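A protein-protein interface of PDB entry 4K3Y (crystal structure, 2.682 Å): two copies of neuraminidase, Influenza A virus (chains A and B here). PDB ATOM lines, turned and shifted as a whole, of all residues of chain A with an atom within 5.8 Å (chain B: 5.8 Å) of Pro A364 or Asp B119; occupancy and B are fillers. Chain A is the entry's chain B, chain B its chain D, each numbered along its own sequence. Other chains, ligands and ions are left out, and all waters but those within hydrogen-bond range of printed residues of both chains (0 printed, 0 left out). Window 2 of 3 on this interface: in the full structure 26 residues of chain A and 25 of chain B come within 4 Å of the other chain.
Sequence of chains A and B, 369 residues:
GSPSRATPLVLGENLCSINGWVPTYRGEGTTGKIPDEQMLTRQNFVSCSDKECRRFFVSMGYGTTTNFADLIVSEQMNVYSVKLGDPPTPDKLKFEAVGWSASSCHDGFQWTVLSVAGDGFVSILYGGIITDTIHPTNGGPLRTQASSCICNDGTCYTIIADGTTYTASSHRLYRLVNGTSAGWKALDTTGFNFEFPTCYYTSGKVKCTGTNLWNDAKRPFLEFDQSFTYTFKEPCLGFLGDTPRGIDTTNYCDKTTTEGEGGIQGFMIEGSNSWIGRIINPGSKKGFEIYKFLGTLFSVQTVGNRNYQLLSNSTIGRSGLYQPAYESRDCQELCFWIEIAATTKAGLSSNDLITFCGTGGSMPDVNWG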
ATOM      1  N   ARG A 306       6.700 -37.087  20.231  1.00  0.00           N
ATOM      2  CA  ARG A 306       7.021 -36.322  21.437  1.00  0.00           C
ATOM      3  C   ARG A 306       7.011 -37.164  22.722  1.00  0.00           C
ATOM      4  O   ARG A 306       6.042 -37.885  23.011  1.00  0.00           O
ATOM      5  CB  ARG A 306       6.022 -35.177  21.582  1.00  0.00           C
ATOM      6  CG  ARG A 306       6.341 -34.204  22.699  1.00  0.00           C
ATOM      7  CD  ARG A 306       7.254 -33.084  22.210  1.00  0.00           C
ATOM      8  NE  ARG A 306       6.982 -31.832  22.917  1.00  0.00           N
ATOM      9  CZ  ARG A 306       7.604 -31.459  24.033  1.00  0.00           C
ATOM     10  NH1 ARG A 306       8.540 -32.241  24.568  1.00  0.00           N
ATOM     11  NH2 ARG A 306       7.294 -30.304  24.612  1.00  0.00           N
ATOM     12  N   TYR A 308       7.122 -36.719  26.753  1.00  0.00           N
ATOM     13  CA  TYR A 308       7.003 -35.791  27.873  1.00  0.00           C
ATOM     14  C   TYR A 308       7.493 -36.453  29.167  1.00  0.00           C
ATOM     15  O   TYR A 308       7.013 -37.529  29.553  1.00  0.00           O
ATOM     16  CB  TYR A 308       5.549 -35.349  28.060  1.00  0.00           C
ATOM     17  CG  TYR A 308       4.951 -34.424  27.009  1.00  0.00           C
ATOM     18  CD1 TYR A 308       5.200 -33.052  27.041  1.00  0.00           C
ATOM     19  CD2 TYR A 308       4.075 -34.912  26.028  1.00  0.00           C
ATOM     20  CE1 TYR A 308       4.626 -32.191  26.105  1.00  0.00           C
ATOM     21  CE2 TYR A 308       3.498 -34.061  25.084  1.00  0.00           C
ATOM     22  CZ  TYR A 308       3.780 -32.701  25.129  1.00  0.00           C
ATOM     23  OH  TYR A 308       3.215 -31.845  24.215  1.00  0.00           O
ATOM     24  N   SER A 362       0.261 -28.367  21.925  1.00  0.00           N
ATOM     25  CA  SER A 362       1.534 -28.914  22.378  1.00  0.00           C
ATOM     26  C   SER A 362       2.016 -28.145  23.614  1.00  0.00           C
ATOM     27  O   SER A 362       1.632 -26.988  23.833  1.00  0.00           O
ATOM     28  CB  SER A 362       2.580 -28.857  21.268  1.00  0.00           C
ATOM     29  OG  SER A 362       3.828 -29.343  21.742  1.00  0.00           O
ATOM     30  N   MET A 363       2.845 -28.785  24.428  1.00  0.00           N
ATOM     31  CA  MET A 363       3.265 -28.180  25.686  1.00  0.00           C
ATOM     32  C   MET A 363       4.779 -28.148  25.844  1.00  0.00           C
ATOM     33  O   MET A 363       5.485 -28.984  25.285  1.00  0.00           O
ATOM     34  CB  MET A 363       2.631 -28.939  26.854  1.00  0.00           C
ATOM     35  CG  MET A 363       1.102 -28.909  26.847  1.00  0.00           C
ATOM     36  SD  MET A 363       0.444 -27.296  27.313  1.00  0.00           S
ATOM     37  CE  MET A 363       1.159 -27.257  28.944  1.00  0.00           C
ATOM     38  N   PRO A 364       5.285 -27.166  26.602  1.00  0.00           N
ATOM     39  CA  PRO A 364       6.713 -27.083  26.946  1.00  0.00           C
ATOM     40  C   PRO A 364       7.089 -28.176  27.938  1.00  0.00           C
ATOM     41  O   PRO A 364       6.198 -28.675  28.631  1.00  0.00           O
ATOM     42  CB  PRO A 364       6.819 -25.719  27.638  1.00  0.00           C
ATOM     43  CG  PRO A 364       5.441 -25.498  28.226  1.00  0.00           C
ATOM     44  CD  PRO A 364       4.507 -26.056  27.186  1.00  0.00           C
ATOM     45  N   ASP A 365       8.371 -28.525  28.016  1.00  0.00           N
ATOM     46  CA  ASP A 365       8.840 -29.567  28.939  1.00  0.00           C
ATOM     47  C   ASP A 365       8.969 -29.097  30.399  1.00  0.00           C
ATOM     48  O   ASP A 365      10.047 -28.666  30.829  1.00  0.00           O
ATOM     49  CB  ASP A 365      10.177 -30.142  28.453  1.00  0.00           C
ATOM     50  CG  ASP A 365      10.082 -30.741  27.061  1.00  0.00           C
ATOM     51  OD1 ASP A 365       9.051 -31.382  26.763  1.00  0.00           O
ATOM     52  OD2 ASP A 365      11.033 -30.572  26.262  1.00  0.00           O
ATOM     53  N   VAL A 366       7.883 -29.201  31.163  1.00  0.00           N
ATOM     54  CA  VAL A 366       7.904 -28.820  32.580  1.00  0.00           C
ATOM     55  C   VAL A 366       7.871 -30.016  33.549  1.00  0.00           C
ATOM     56  O   VAL A 366       7.257 -31.037  33.255  1.00  0.00           O
ATOM     57  CB  VAL A 366       6.820 -27.730  32.907  1.00  0.00           C
ATOM     58  CG1 VAL A 366       5.791 -27.634  31.803  1.00  0.00           C
ATOM     59  CG2 VAL A 366       6.166 -27.931  34.277  1.00  0.00           C
ATOM     60  N   TRP B 100       1.759 -19.997  40.188  1.00  0.00           N
ATOM     61  CA  TRP B 100       2.256 -18.955  41.094  1.00  0.00           C
ATOM     62  C   TRP B 100       1.534 -17.626  40.864  1.00  0.00           C
ATOM     63  O   TRP B 100       1.870 -16.612  41.474  1.00  0.00           O
ATOM     64  CB  TRP B 100       3.772 -18.758  40.905  1.00  0.00           C
ATOM     65  CG  TRP B 100       4.158 -18.460  39.487  1.00  0.00           C
ATOM     66  CD1 TRP B 100       3.969 -17.288  38.809  1.00  0.00           C
ATOM     67  CD2 TRP B 100       4.787 -19.357  38.572  1.00  0.00           C
ATOM     68  NE1 TRP B 100       4.447 -17.402  37.527  1.00  0.00           N
ATOM     69  CE2 TRP B 100       4.958 -18.661  37.354  1.00  0.00           C
ATOM     70  CE3 TRP B 100       5.230 -20.682  38.665  1.00  0.00           C
ATOM     71  CZ2 TRP B 100       5.553 -19.249  36.230  1.00  0.00           C
ATOM     72  CZ3 TRP B 100       5.825 -21.262  37.549  1.00  0.00           C
ATOM     73  CH2 TRP B 100       5.981 -20.544  36.348  1.00  0.00           C
ATOM     74  N   ALA B 117       1.878 -21.343  35.119  1.00  0.00           N
ATOM     75  CA  ALA B 117       2.609 -22.476  35.643  1.00  0.00           C
ATOM     76  C   ALA B 117       3.689 -22.850  34.644  1.00  0.00           C
ATOM     77  O   ALA B 117       3.795 -22.236  33.573  1.00  0.00           O
ATOM     78  CB  ALA B 117       1.663 -23.640  35.875  1.00  0.00           C
ATOM     79  N   GLY B 118       4.489 -23.851  35.004  1.00  0.00           N
ATOM     80  CA  GLY B 118       5.562 -24.330  34.153  1.00  0.00           C
ATOM     81  C   GLY B 118       6.629 -23.282  33.906  1.00  0.00           C
ATOM     82  O   GLY B 118       7.284 -22.809  34.835  1.00  0.00           O
ATOM     83  N   ASP B 119       6.797 -22.912  32.642  1.00  0.00           N
ATOM     84  CA  ASP B 119       7.801 -21.931  32.260  1.00  0.00           C
ATOM     85  C   ASP B 119       7.209 -20.523  32.188  1.00  0.00           C
ATOM     86  O   ASP B 119       7.942 -19.540  32.032  1.00  0.00           O
ATOM     87  CB  ASP B 119       8.472 -22.325  30.936  1.00  0.00           C
ATOM     88  CG  ASP B 119       7.509 -22.317  29.748  1.00  0.00           C
ATOM     89  OD1 ASP B 119       6.294 -22.529  29.945  1.00  0.00           O
ATOM     90  OD2 ASP B 119       7.978 -22.105  28.605  1.00  0.00           O
ATOM     91  N   GLY B 120       5.886 -20.433  32.312  1.00  0.00           N
ATOM     92  CA  GLY B 120       5.203 -19.151  32.261  1.00  0.00           C
ATOM     93  C   GLY B 120       4.065 -19.077  31.255  1.00  0.00           C
ATOM     94  O   GLY B 120       3.748 -18.001  30.738  1.00  0.00           O
ATOM     95  N   PHE B 121       3.450 -20.220  30.965  1.00  0.00           N
ATOM     96  CA  PHE B 121       2.220 -20.230  30.178  1.00  0.00           C
ATOM     97  C   PHE B 121       1.021 -20.256  31.126  1.00  0.00           C
ATOM     98  O   PHE B 121       1.126 -20.746  32.259  1.00  0.00           O
ATOM     99  CB  PHE B 121       2.175 -21.449  29.253  1.00  0.00           C
ATOM    100  CG  PHE B 121       2.115 -22.763  29.983  1.00  0.00           C
ATOM    101  CD1 PHE B 121       3.279 -23.362  30.455  1.00  0.00           C
ATOM    102  CD2 PHE B 121       0.896 -23.395  30.201  1.00  0.00           C
ATOM    103  CE1 PHE B 121       3.229 -24.564  31.131  1.00  0.00           C
ATOM    104  CE2 PHE B 121       0.840 -24.589  30.879  1.00  0.00           C
ATOM    105  CZ  PHE B 121       2.010 -25.177  31.349  1.00  0.00           C
ATOM    106  N   HIS B 135      -0.027 -19.127  25.631  1.00  0.00           N
ATOM    107  CA  HIS B 135       1.422 -19.142  25.738  1.00  0.00           C
ATOM    108  C   HIS B 135       2.031 -17.779  25.449  1.00  0.00           C
ATOM    109  O   HIS B 135       1.486 -16.995  24.671  1.00  0.00           O
ATOM    110  CB  HIS B 135       2.013 -20.226  24.835  1.00  0.00           C
ATOM    111  CG  HIS B 135       1.652 -21.619  25.257  1.00  0.00           C
ATOM    112  ND1 HIS B 135       2.444 -22.368  26.102  1.00  0.00           N
ATOM    113  CD2 HIS B 135       0.581 -22.389  24.958  1.00  0.00           C
ATOM    114  CE1 HIS B 135       1.878 -23.546  26.296  1.00  0.00           C
ATOM    115  NE2 HIS B 135       0.747 -23.586  25.619  1.00  0.00           N
ATOM    116  N   PRO B 136       3.154 -17.481  26.115  1.00  0.00           N
ATOM    117  CA  PRO B 136       3.922 -16.258  25.871  1.00  0.00           C
ATOM    118  C   PRO B 136       4.437 -16.171  24.435  1.00  0.00           C
ATOM    119  O   PRO B 136       4.964 -17.158  23.912  1.00  0.00           O
ATOM    120  CB  PRO B 136       5.109 -16.400  26.832  1.00  0.00           C
ATOM    121  CG  PRO B 136       5.161 -17.861  27.192  1.00  0.00           C
ATOM    122  CD  PRO B 136       3.739 -18.300  27.192  1.00  0.00           C
ATOM    123  N   PRO B 141       7.648 -14.271  31.209  1.00  0.00           N
ATOM    124  CA  PRO B 141       6.508 -15.152  31.482  1.00  0.00           C
ATOM    125  C   PRO B 141       5.185 -14.377  31.404  1.00  0.00           C
ATOM    126  O   PRO B 141       5.187 -13.142  31.475  1.00  0.00           O
ATOM    127  CB  PRO B 141       6.760 -15.608  32.927  1.00  0.00           C
ATOM    128  CG  PRO B 141       7.644 -14.559  33.524  1.00  0.00           C
ATOM    129  CD  PRO B 141       8.510 -14.086  32.392  1.00  0.00           C
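Pro A364 touches just these residues of chain B: Asp B119 (3.5 Å), Phe B121 (3.8 Å) and His B135 (3.7 Å).
Of the printed residues of chain A, Asp B119 touches Pro A364 (3.5 Å).
Printed residues of chain B within 4 Å of Val A366: Gly B118.
Printed residues of chain B within 4 Å of Met A363: Phe B121.
Of the printed residues of chain A, Gly B118 touches Val A366 (3.7 Å).
Printed residues of chain B within 4 Å of Ser A362: His B135 (3.9 Å).
Pro B141 touches none of the printed residues of chain A.
Pro B136 touches none of the printed residues of chain A.
The nearest printed residue of chain B that does not touch Pro A364 is Gly B118 (6.0 Å).
The nearest residue of chain A that does not touch Asp B119 is Val A366 (4.8 Å).
Among the printed residues, pairs that only touch across the chains: Ser A362 with His B135 (3.9 Å), Met A363 with Phe B121 (3.3 Å), Pro A364 with Asp B119 (3.5 Å), Pro A364 with Phe B121 (3.8 Å), Pro A364 with His B135 (3.7 Å) and Val A366 with Gly B118 (3.7 Å).
Hydrophobic or aromatic side chains of chain A within 4 Å of the printed part of chain B: Met A363, Pro A364 and Val A366.
Of the 9 printed residues of chain B, 4 touch a printed residue of chain A.
Hydrophobic or aromatic side chains of chain B that line the printed part of chain A: Phe B121 and His B135.
No position is printed for both chains.
Of the 6 pairs that touch across the chains among the printed residues, none has its exchanged pair printed and touching as well.
OH of Tyr A308 sits at hydrogen-bond distance from N of Met A363, at 3.1 Å.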
